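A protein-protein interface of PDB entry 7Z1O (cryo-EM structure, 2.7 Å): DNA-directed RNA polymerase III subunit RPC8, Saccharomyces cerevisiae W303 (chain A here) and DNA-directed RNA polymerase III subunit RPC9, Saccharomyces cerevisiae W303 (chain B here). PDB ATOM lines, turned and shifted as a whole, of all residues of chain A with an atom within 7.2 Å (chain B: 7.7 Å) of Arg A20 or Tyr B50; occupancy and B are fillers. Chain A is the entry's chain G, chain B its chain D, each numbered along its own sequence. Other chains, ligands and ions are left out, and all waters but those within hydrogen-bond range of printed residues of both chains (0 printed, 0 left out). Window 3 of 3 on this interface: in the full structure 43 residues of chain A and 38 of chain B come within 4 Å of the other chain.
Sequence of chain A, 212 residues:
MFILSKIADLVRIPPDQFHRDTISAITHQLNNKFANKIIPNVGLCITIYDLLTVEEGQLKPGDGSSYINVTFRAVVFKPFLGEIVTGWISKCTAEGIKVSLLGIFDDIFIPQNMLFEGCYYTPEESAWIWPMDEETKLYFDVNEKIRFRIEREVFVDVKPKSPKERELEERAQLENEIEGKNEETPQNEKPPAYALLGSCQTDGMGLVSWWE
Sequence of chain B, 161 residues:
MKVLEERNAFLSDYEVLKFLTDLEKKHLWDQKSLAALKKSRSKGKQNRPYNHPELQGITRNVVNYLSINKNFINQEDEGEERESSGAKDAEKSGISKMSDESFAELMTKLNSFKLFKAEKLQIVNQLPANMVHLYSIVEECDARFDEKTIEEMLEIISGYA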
ATOM      1  N   ASP A  16      14.723  -5.573  -0.384  1.00  0.00           N
ATOM      2  CA  ASP A  16      16.159  -5.328  -0.416  1.00  0.00           C
ATOM      3  C   ASP A  16      16.964  -6.409   0.295  1.00  0.00           C
ATOM      4  O   ASP A  16      18.189  -6.441   0.146  1.00  0.00           O
ATOM      5  CB  ASP A  16      16.473  -3.939   0.160  1.00  0.00           C
ATOM      6  CG  ASP A  16      16.077  -3.790   1.622  1.00  0.00           C
ATOM      7  OD1 ASP A  16      15.515  -4.731   2.215  1.00  0.00           O
ATOM      8  OD2 ASP A  16      16.332  -2.706   2.186  1.00  0.00           O
ATOM      9  N   GLN A  17      16.312  -7.286   1.054  1.00  0.00           N
ATOM     10  CA  GLN A  17      16.965  -8.417   1.697  1.00  0.00           C
ATOM     11  C   GLN A  17      16.867  -9.696   0.880  1.00  0.00           C
ATOM     12  O   GLN A  17      17.211 -10.767   1.391  1.00  0.00           O
ATOM     13  CB  GLN A  17      16.367  -8.658   3.086  1.00  0.00           C
ATOM     14  CG  GLN A  17      16.217  -7.409   3.927  1.00  0.00           C
ATOM     15  CD  GLN A  17      17.403  -7.176   4.834  1.00  0.00           C
ATOM     16  OE1 GLN A  17      18.328  -7.984   4.882  1.00  0.00           O
ATOM     17  NE2 GLN A  17      17.381  -6.067   5.563  1.00  0.00           N
ATOM     18  N   PHE A  18      16.396  -9.616  -0.366  1.00  0.00           N
ATOM     19  CA  PHE A  18      16.254 -10.814  -1.188  1.00  0.00           C
ATOM     20  C   PHE A  18      17.605 -11.389  -1.590  1.00  0.00           C
ATOM     21  O   PHE A  18      17.697 -12.580  -1.907  1.00  0.00           O
ATOM     22  CB  PHE A  18      15.424 -10.505  -2.432  1.00  0.00           C
ATOM     23  CG  PHE A  18      13.950 -10.366  -2.167  1.00  0.00           C
ATOM     24  CD1 PHE A  18      13.409 -10.739  -0.950  1.00  0.00           C
ATOM     25  CD2 PHE A  18      13.106  -9.869  -3.144  1.00  0.00           C
ATOM     26  CE1 PHE A  18      12.057 -10.611  -0.710  1.00  0.00           C
ATOM     27  CE2 PHE A  18      11.752  -9.742  -2.907  1.00  0.00           C
ATOM     28  CZ  PHE A  18      11.228 -10.112  -1.690  1.00  0.00           C
ATOM     29  N   HIS A  19      18.658 -10.567  -1.594  1.00  0.00           N
ATOM     30  CA  HIS A  19      19.983 -11.068  -1.940  1.00  0.00           C
ATOM     31  C   HIS A  19      20.528 -12.001  -0.868  1.00  0.00           C
ATOM     32  O   HIS A  19      21.320 -12.899  -1.175  1.00  0.00           O
ATOM     33  CB  HIS A  19      20.945  -9.902  -2.171  1.00  0.00           C
ATOM     34  CG  HIS A  19      21.284  -9.137  -0.930  1.00  0.00           C
ATOM     35  ND1 HIS A  19      20.554  -8.048  -0.503  1.00  0.00           N
ATOM     36  CD2 HIS A  19      22.282  -9.296  -0.028  1.00  0.00           C
ATOM     37  CE1 HIS A  19      21.085  -7.575   0.611  1.00  0.00           C
ATOM     38  NE2 HIS A  19      22.133  -8.314   0.919  1.00  0.00           N
ATOM     39  N   ARG A  20      20.122 -11.807   0.383  1.00  0.00           N
ATOM     40  CA  ARG A  20      20.548 -12.678   1.464  1.00  0.00           C
ATOM     41  C   ARG A  20      19.883 -14.045   1.343  1.00  0.00           C
ATOM     42  O   ARG A  20      18.892 -14.225   0.631  1.00  0.00           O
ATOM     43  CB  ARG A  20      20.207 -12.056   2.818  1.00  0.00           C
ATOM     44  CG  ARG A  20      21.209 -11.030   3.309  1.00  0.00           C
ATOM     45  CD  ARG A  20      20.732 -10.382   4.596  1.00  0.00           C
ATOM     46  NE  ARG A  20      21.381 -10.949   5.772  1.00  0.00           N
ATOM     47  CZ  ARG A  20      21.575 -10.294   6.909  1.00  0.00           C
ATOM     48  NH1 ARG A  20      21.178  -9.042   7.062  1.00  0.00           N
ATOM     49  NH2 ARG A  20      22.183 -10.912   7.918  1.00  0.00           N
ATOM     50  N   ASP A  21      20.453 -15.020   2.046  1.00  0.00           N
ATOM     51  CA  ASP A  21      19.818 -16.324   2.154  1.00  0.00           C
ATOM     52  C   ASP A  21      18.501 -16.191   2.906  1.00  0.00           C
ATOM     53  O   ASP A  21      18.368 -15.361   3.811  1.00  0.00           O
ATOM     54  CB  ASP A  21      20.743 -17.311   2.865  1.00  0.00           C
ATOM     55  CG  ASP A  21      20.382 -18.756   2.583  1.00  0.00           C
ATOM     56  OD1 ASP A  21      19.397 -18.995   1.854  1.00  0.00           O
ATOM     57  OD2 ASP A  21      21.087 -19.655   3.089  1.00  0.00           O
ATOM     58  N   THR A  22      17.517 -17.004   2.514  1.00  0.00           N
ATOM     59  CA  THR A  22      16.179 -16.873   3.084  1.00  0.00           C
ATOM     60  C   THR A  22      16.167 -17.231   4.565  1.00  0.00           C
ATOM     61  O   THR A  22      15.457 -16.597   5.356  1.00  0.00           O
ATOM     62  CB  THR A  22      15.191 -17.745   2.314  1.00  0.00           C
ATOM     63  OG1 THR A  22      15.448 -17.628   0.909  1.00  0.00           O
ATOM     64  CG2 THR A  22      13.770 -17.295   2.591  1.00  0.00           C
ATOM     65  N   ILE A  23      16.948 -18.240   4.958  1.00  0.00           N
ATOM     66  CA  ILE A  23      17.055 -18.605   6.370  1.00  0.00           C
ATOM     67  C   ILE A  23      17.621 -17.441   7.174  1.00  0.00           C
ATOM     68  O   ILE A  23      17.114 -17.102   8.250  1.00  0.00           O
ATOM     69  CB  ILE A  23      17.913 -19.872   6.533  1.00  0.00           C
ATOM     70  CG1 ILE A  23      17.238 -21.072   5.862  1.00  0.00           C
ATOM     71  CG2 ILE A  23      18.200 -20.149   8.004  1.00  0.00           C
ATOM     72  CD1 ILE A  23      16.174 -21.734   6.710  1.00  0.00           C
ATOM     73  N   SER A  24      18.670 -16.803   6.649  1.00  0.00           N
ATOM     74  CA  SER A  24      19.288 -15.680   7.347  1.00  0.00           C
ATOM     75  C   SER A  24      18.336 -14.496   7.455  1.00  0.00           C
ATOM     76  O   SER A  24      18.272 -13.842   8.500  1.00  0.00           O
ATOM     77  CB  SER A  24      20.577 -15.270   6.639  1.00  0.00           C
ATOM     78  OG  SER A  24      21.220 -14.212   7.327  1.00  0.00           O
ATOM     79  N   ALA A  25      17.584 -14.206   6.389  1.00  0.00           N
ATOM     80  CA  ALA A  25      16.643 -13.089   6.427  1.00  0.00           C
ATOM     81  C   ALA A  25      15.506 -13.348   7.409  1.00  0.00           C
ATOM     82  O   ALA A  25      15.115 -12.452   8.173  1.00  0.00           O
ATOM     83  CB  ALA A  25      16.093 -12.821   5.028  1.00  0.00           C
ATOM     84  N   THR A  27      15.627 -15.352  10.024  1.00  0.00           N
ATOM     85  CA  THR A  27      16.201 -15.299  11.364  1.00  0.00           C
ATOM     86  C   THR A  27      16.462 -13.863  11.799  1.00  0.00           C
ATOM     87  O   THR A  27      16.271 -13.519  12.969  1.00  0.00           O
ATOM     88  CB  THR A  27      17.490 -16.120  11.415  1.00  0.00           C
ATOM     89  OG1 THR A  27      17.266 -17.397  10.805  1.00  0.00           O
ATOM     90  CG2 THR A  27      17.932 -16.330  12.851  1.00  0.00           C
ATOM     91  N   HIS A  28      16.888 -13.006  10.867  1.00  0.00           N
ATOM     92  CA  HIS A  28      17.115 -11.603  11.197  1.00  0.00           C
ATOM     93  C   HIS A  28      15.817 -10.907  11.580  1.00  0.00           C
ATOM     94  O   HIS A  28      15.772 -10.169  12.572  1.00  0.00           O
ATOM     95  CB  HIS A  28      17.776 -10.888  10.022  1.00  0.00           C
ATOM     96  CG  HIS A  28      17.971  -9.421  10.240  1.00  0.00           C
ATOM     97  ND1 HIS A  28      18.547  -8.910  11.383  1.00  0.00           N
ATOM     98  CD2 HIS A  28      17.669  -8.355   9.463  1.00  0.00           C
ATOM     99  CE1 HIS A  28      18.591  -7.593  11.301  1.00  0.00           C
ATOM    100  NE2 HIS A  28      18.064  -7.231  10.145  1.00  0.00           N
ATOM    101  N   GLN A  29      14.747 -11.135  10.814  1.00  0.00           N
ATOM    102  CA  GLN A  29      13.457 -10.539  11.157  1.00  0.00           C
ATOM    103  C   GLN A  29      12.938 -11.072  12.489  1.00  0.00           C
ATOM    104  O   GLN A  29      12.385 -10.317  13.302  1.00  0.00           O
ATOM    105  CB  GLN A  29      12.444 -10.796  10.044  1.00  0.00           C
ATOM    106  CG  GLN A  29      12.809 -10.164   8.718  1.00  0.00           C
ATOM    107  CD  GLN A  29      12.831  -8.652   8.785  1.00  0.00           C
ATOM    108  OE1 GLN A  29      11.947  -8.035   9.376  1.00  0.00           O
ATOM    109  NE2 GLN A  29      13.844  -8.047   8.180  1.00  0.00           N
ATOM    110  N   ASN A  31      14.765 -12.068  14.934  1.00  0.00           N
ATOM    111  CA  ASN A  31      15.579 -11.495  15.999  1.00  0.00           C
ATOM    112  C   ASN A  31      15.222 -10.034  16.241  1.00  0.00           C
ATOM    113  O   ASN A  31      15.338  -9.541  17.368  1.00  0.00           O
ATOM    114  CB  ASN A  31      17.061 -11.644  15.664  1.00  0.00           C
ATOM    115  CG  ASN A  31      17.582 -13.037  15.954  1.00  0.00           C
ATOM    116  OD1 ASN A  31      17.154 -13.686  16.905  1.00  0.00           O
ATOM    117  ND2 ASN A  31      18.517 -13.500  15.134  1.00  0.00           N
ATOM    118  N   ASN A  32      14.803  -9.319  15.193  1.00  0.00           N
ATOM    119  CA  ASN A  32      14.238  -7.988  15.407  1.00  0.00           C
ATOM    120  C   ASN A  32      12.970  -8.062  16.246  1.00  0.00           C
ATOM    121  O   ASN A  32      12.761  -7.239  17.145  1.00  0.00           O
ATOM    122  CB  ASN A  32      13.936  -7.284  14.081  1.00  0.00           C
ATOM    123  CG  ASN A  32      15.179  -6.961  13.282  1.00  0.00           C
ATOM    124  OD1 ASN A  32      15.388  -7.486  12.191  1.00  0.00           O
ATOM    125  ND2 ASN A  32      16.000  -6.066  13.810  1.00  0.00           N
ATOM    126  N   LEU B  23      27.331 -18.656  17.617  1.00  0.00           N
ATOM    127  CA  LEU B  23      26.675 -17.508  16.999  1.00  0.00           C
ATOM    128  C   LEU B  23      27.587 -16.286  16.986  1.00  0.00           C
ATOM    129  O   LEU B  23      27.635 -15.547  15.995  1.00  0.00           O
ATOM    130  CB  LEU B  23      25.374 -17.195  17.734  1.00  0.00           C
ATOM    131  CG  LEU B  23      24.406 -16.229  17.053  1.00  0.00           C
ATOM    132  CD1 LEU B  23      23.570 -16.960  16.019  1.00  0.00           C
ATOM    133  CD2 LEU B  23      23.521 -15.550  18.082  1.00  0.00           C
ATOM    134  N   LYS B  26      30.155 -16.803  14.344  1.00  0.00           N
ATOM    135  CA  LYS B  26      29.582 -16.649  13.010  1.00  0.00           C
ATOM    136  C   LYS B  26      29.350 -15.184  12.665  1.00  0.00           C
ATOM    137  O   LYS B  26      29.609 -14.757  11.534  1.00  0.00           O
ATOM    138  CB  LYS B  26      28.275 -17.435  12.914  1.00  0.00           C
ATOM    139  CG  LYS B  26      27.654 -17.453  11.529  1.00  0.00           C
ATOM    140  CD  LYS B  26      26.327 -18.192  11.537  1.00  0.00           C
ATOM    141  CE  LYS B  26      26.534 -19.692  11.665  1.00  0.00           C
ATOM    142  NZ  LYS B  26      25.252 -20.440  11.556  1.00  0.00           N
ATOM    143  N   HIS B  27      28.866 -14.398  13.623  1.00  0.00           N
ATOM    144  CA  HIS B  27      28.572 -12.991  13.391  1.00  0.00           C
ATOM    145  C   HIS B  27      29.743 -12.075  13.715  1.00  0.00           C
ATOM    146  O   HIS B  27      29.580 -10.852  13.654  1.00  0.00           O
ATOM    147  CB  HIS B  27      27.348 -12.565  14.207  1.00  0.00           C
ATOM    148  CG  HIS B  27      26.056 -13.120  13.693  1.00  0.00           C
ATOM    149  ND1 HIS B  27      25.266 -13.972  14.433  1.00  0.00           N
ATOM    150  CD2 HIS B  27      25.422 -12.951  12.510  1.00  0.00           C
ATOM    151  CE1 HIS B  27      24.197 -14.300  13.731  1.00  0.00           C
ATOM    152  NE2 HIS B  27      24.268 -13.694  12.559  1.00  0.00           N
ATOM    153  N   LEU B  28      30.905 -12.640  14.060  1.00  0.00           N
ATOM    154  CA  LEU B  28      32.111 -11.888  14.420  1.00  0.00           C
ATOM    155  C   LEU B  28      31.839 -10.951  15.600  1.00  0.00           C
ATOM    156  O   LEU B  28      31.966  -9.729  15.506  1.00  0.00           O
ATOM    157  CB  LEU B  28      32.678 -11.121  13.216  1.00  0.00           C
ATOM    158  CG  LEU B  28      33.584 -11.839  12.205  1.00  0.00           C
ATOM    159  CD1 LEU B  28      34.874 -12.298  12.874  1.00  0.00           C
ATOM    160  CD2 LEU B  28      32.894 -12.999  11.496  1.00  0.00           C
ATOM    161  N   TRP B  29      31.459 -11.558  16.724  1.00  0.00           N
ATOM    162  CA  TRP B  29      31.108 -10.821  17.928  1.00  0.00           C
ATOM    163  C   TRP B  29      32.013 -11.106  19.117  1.00  0.00           C
ATOM    164  O   TRP B  29      31.820 -10.491  20.172  1.00  0.00           O
ATOM    165  CB  TRP B  29      29.659 -11.124  18.339  1.00  0.00           C
ATOM    166  CG  TRP B  29      28.641 -10.240  17.697  1.00  0.00           C
ATOM    167  CD1 TRP B  29      28.855  -9.023  17.122  1.00  0.00           C
ATOM    168  CD2 TRP B  29      27.239 -10.501  17.574  1.00  0.00           C
ATOM    169  NE1 TRP B  29      27.674  -8.512  16.643  1.00  0.00           N
ATOM    170  CE2 TRP B  29      26.666  -9.402  16.909  1.00  0.00           C
ATOM    171  CE3 TRP B  29      26.413 -11.560  17.959  1.00  0.00           C
ATOM    172  CZ2 TRP B  29      25.307  -9.330  16.623  1.00  0.00           C
ATOM    173  CZ3 TRP B  29      25.065 -11.488  17.674  1.00  0.00           C
ATOM    174  CH2 TRP B  29      24.525 -10.382  17.012  1.00  0.00           C
ATOM    175  N   LYS B  38      37.896  -4.259  14.768  1.00  0.00           N
ATOM    176  CA  LYS B  38      36.846  -3.299  15.107  1.00  0.00           C
ATOM    177  C   LYS B  38      37.417  -2.079  15.819  1.00  0.00           C
ATOM    178  O   LYS B  38      36.945  -0.954  15.610  1.00  0.00           O
ATOM    179  CB  LYS B  38      35.764  -3.966  15.963  1.00  0.00           C
ATOM    180  CG  LYS B  38      34.693  -4.725  15.177  1.00  0.00           C
ATOM    181  CD  LYS B  38      35.201  -6.048  14.622  1.00  0.00           C
ATOM    182  CE  LYS B  38      34.091  -6.825  13.937  1.00  0.00           C
ATOM    183  NZ  LYS B  38      34.595  -8.068  13.291  1.00  0.00           N
ATOM    184  N   ARG B  48      32.608  -6.277   8.196  1.00  0.00           N
ATOM    185  CA  ARG B  48      31.770  -5.597   9.166  1.00  0.00           C
ATOM    186  C   ARG B  48      31.090  -6.607  10.080  1.00  0.00           C
ATOM    187  O   ARG B  48      30.760  -7.719   9.646  1.00  0.00           O
ATOM    188  CB  ARG B  48      30.704  -4.742   8.461  1.00  0.00           C
ATOM    189  CG  ARG B  48      31.197  -3.397   7.940  1.00  0.00           C
ATOM    190  CD  ARG B  48      31.833  -3.526   6.563  1.00  0.00           C
ATOM    191  NE  ARG B  48      30.956  -4.201   5.613  1.00  0.00           N
ATOM    192  CZ  ARG B  48      30.011  -3.599   4.904  1.00  0.00           C
ATOM    193  NH1 ARG B  48      29.790  -2.299   5.009  1.00  0.00           N
ATOM    194  NH2 ARG B  48      29.270  -4.320   4.067  1.00  0.00           N
ATOM    195  N   PRO B  49      30.866  -6.253  11.342  1.00  0.00           N
ATOM    196  CA  PRO B  49      30.119  -7.144  12.234  1.00  0.00           C
ATOM    197  C   PRO B  49      28.624  -7.073  11.964  1.00  0.00           C
ATOM    198  O   PRO B  49      28.135  -6.247  11.190  1.00  0.00           O
ATOM    199  CB  PRO B  49      30.455  -6.610  13.628  1.00  0.00           C
ATOM    200  CG  PRO B  49      30.718  -5.162  13.405  1.00  0.00           C
ATOM    201  CD  PRO B  49      31.357  -5.054  12.044  1.00  0.00           C
ATOM    202  N   TYR B  50      27.896  -7.974  12.619  1.00  0.00           N
ATOM    203  CA  TYR B  50      26.443  -7.969  12.527  1.00  0.00           C
ATOM    204  C   TYR B  50      25.890  -6.740  13.241  1.00  0.00           C
ATOM    205  O   TYR B  50      26.265  -6.439  14.377  1.00  0.00           O
ATOM    206  CB  TYR B  50      25.882  -9.256  13.131  1.00  0.00           C
ATOM    207  CG  TYR B  50      24.454  -9.573  12.753  1.00  0.00           C
ATOM    208  CD1 TYR B  50      24.129  -9.955  11.458  1.00  0.00           C
ATOM    209  CD2 TYR B  50      23.437  -9.521  13.696  1.00  0.00           C
ATOM    210  CE1 TYR B  50      22.828 -10.258  11.110  1.00  0.00           C
ATOM    211  CE2 TYR B  50      22.135  -9.824  13.357  1.00  0.00           C
ATOM    212  CZ  TYR B  50      21.836 -10.190  12.065  1.00  0.00           C
ATOM    213  OH  TYR B  50      20.538 -10.490  11.728  1.00  0.00           O
ATOM    214  N   ASN B  51      24.991  -6.027  12.561  1.00  0.00           N
ATOM    215  CA  ASN B  51      24.618  -4.680  12.986  1.00  0.00           C
ATOM    216  C   ASN B  51      23.715  -4.675  14.215  1.00  0.00           C
ATOM    217  O   ASN B  51      23.727  -3.701  14.975  1.00  0.00           O
ATOM    218  CB  ASN B  51      23.933  -3.948  11.829  1.00  0.00           C
ATOM    219  CG  ASN B  51      24.099  -2.438  11.902  1.00  0.00           C
ATOM    220  OD1 ASN B  51      24.277  -1.865  12.976  1.00  0.00           O
ATOM    221  ND2 ASN B  51      24.042  -1.785  10.747  1.00  0.00           N
ATOM    222  N   HIS B  52      22.939  -5.742  14.431  1.00  0.00           N
ATOM    223  CA  HIS B  52      21.895  -5.781  15.452  1.00  0.00           C
ATOM    224  C   HIS B  52      22.465  -5.597  16.855  1.00  0.00           C
ATOM    225  O   HIS B  52      23.213  -6.455  17.342  1.00  0.00           O
ATOM    226  CB  HIS B  52      21.124  -7.098  15.370  1.00  0.00           C
ATOM    227  CG  HIS B  52      19.738  -7.022  15.927  1.00  0.00           C
ATOM    228  ND1 HIS B  52      19.381  -7.605  17.123  1.00  0.00           N
ATOM    229  CD2 HIS B  52      18.620  -6.426  15.452  1.00  0.00           C
ATOM    230  CE1 HIS B  52      18.103  -7.375  17.360  1.00  0.00           C
ATOM    231  NE2 HIS B  52      17.617  -6.662  16.361  1.00  0.00           N
ATOM    232  N   PRO B  53      22.136  -4.492  17.533  1.00  0.00           N
ATOM    233  CA  PRO B  53      22.726  -4.232  18.852  1.00  0.00           C
ATOM    234  C   PRO B  53      22.033  -4.971  19.987  1.00  0.00           C
ATOM    235  O   PRO B  53      22.675  -5.316  20.983  1.00  0.00           O
ATOM    236  CB  PRO B  53      22.575  -2.714  19.001  1.00  0.00           C
ATOM    237  CG  PRO B  53      21.358  -2.385  18.206  1.00  0.00           C
ATOM    238  CD  PRO B  53      21.274  -3.386  17.080  1.00  0.00           C
ATOM    239  N   LEU B  55      20.501  -8.052  20.003  1.00  0.00           N
ATOM    240  CA  LEU B  55      20.929  -9.443  20.077  1.00  0.00           C
ATOM    241  C   LEU B  55      22.370  -9.551  20.552  1.00  0.00           C
ATOM    242  O   LEU B  55      22.704 -10.441  21.342  1.00  0.00           O
ATOM    243  CB  LEU B  55      20.761 -10.121  18.720  1.00  0.00           C
ATOM    244  CG  LEU B  55      21.046 -11.620  18.704  1.00  0.00           C
ATOM    245  CD1 LEU B  55      20.071 -12.335  19.617  1.00  0.00           C
ATOM    246  CD2 LEU B  55      20.965 -12.166  17.291  1.00  0.00           C
ATOM    247  N   GLN B  56      23.237  -8.648  20.086  1.00  0.00           N
ATOM    248  CA  GLN B  56      24.624  -8.641  20.539  1.00  0.00           C
ATOM    249  C   GLN B  56      24.713  -8.372  22.035  1.00  0.00           C
ATOM    250  O   GLN B  56      25.471  -9.039  22.749  1.00  0.00           O
ATOM    251  CB  GLN B  56      25.424  -7.598  19.762  1.00  0.00           C
ATOM    252  CG  GLN B  56      26.914  -7.614  20.045  1.00  0.00           C
ATOM    253  CD  GLN B  56      27.672  -6.592  19.223  1.00  0.00           C
ATOM    254  OE1 GLN B  56      27.075  -5.815  18.477  1.00  0.00           O
ATOM    255  NE2 GLN B  56      28.992  -6.587  19.353  1.00  0.00           N
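The backbone carbonyl oxygen of His B27 sits at hydrogen-bond distance from the backbone NH of Tyr B50 (3.5 Å).
The indole nitrogen (NE1) of Trp B29 is in hydrogen-bond range of the backbone carbonyl oxygen (O) of Tyr B50, at 3.4 Å.
The backbone NH (N) of Leu B55 is in hydrogen-bond range of a ring nitrogen (ND1) of His B52 (3.1 Å).
The guanidinium group (NH2) of Arg A20 lies within hydrogen-bond range of the side-chain hydroxyl (OG) of Ser A24.
The side-chain amide nitrogen (ND2) of Asn A31 is in hydrogen-bond range of the backbone carbonyl oxygen (O) of Thr A27, 3.1 Å away.
The backbone carbonyl oxygen of His A28 lies close to the side-chain amide oxygen of Asn A32 (2.7 Å).
Of the 15 printed residues of chain A, 4 touch a printed residue of chain B.
Hydrophobic or aromatic side chains of chain A within 4 Å of the printed part of chain B: His A28.
Of the 14 printed residues of chain B, 3 touch a printed residue of chain A.
Printed residues of chain B that touch a printed residue of chain A: Tyr B50, His B52 and Leu B55.
Hydrophobic or aromatic side chains of chain B that line the printed part of chain A: Tyr B50, His B52 and Leu B55.
Among the printed residues, 5 pairs touch across the chains.
Among the printed residues, no Asp or Glu carboxylate lies within 4 Å of a Lys or Arg side-chain nitrogen of the other chain.
Tyr B50 touches two residues of chain A.
Of the printed residues of chain B, His A28 touches Tyr B50 (2.6 Å).
Printed residues of chain A within 4 Å of His B52: Asn A31 and Asn A32.
Of the printed residues of chain B, Asn A32 touches His B52 (3.1 Å).
Of the printed residues of chain B, Asn A31 touches His B52 and Leu B55.
Printed residues of chain A within 4 Å of Leu B55: Asn A31 (3.5 Å).
The nearest residue of chain B that does not touch Arg A20 is His B27 (5.8 Å).
The nearest residue of chain A that does not touch Tyr B50 is Asn A31 (5.0 Å).
Arg A20 touches Tyr B50.
Asn A31 touches His B52.
ND2 of Asn A31 touches CD2 of Leu B55, at 3.5 Å.
OH of Tyr B50 is in hydrogen-bond range of ND1 of His A28, 2.6 Å away.
The side-chain amide nitrogen (ND2) of Asn A32 lies within hydrogen-bond range of a ring nitrogen (NE2) of His B52, at 3.1 Å.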
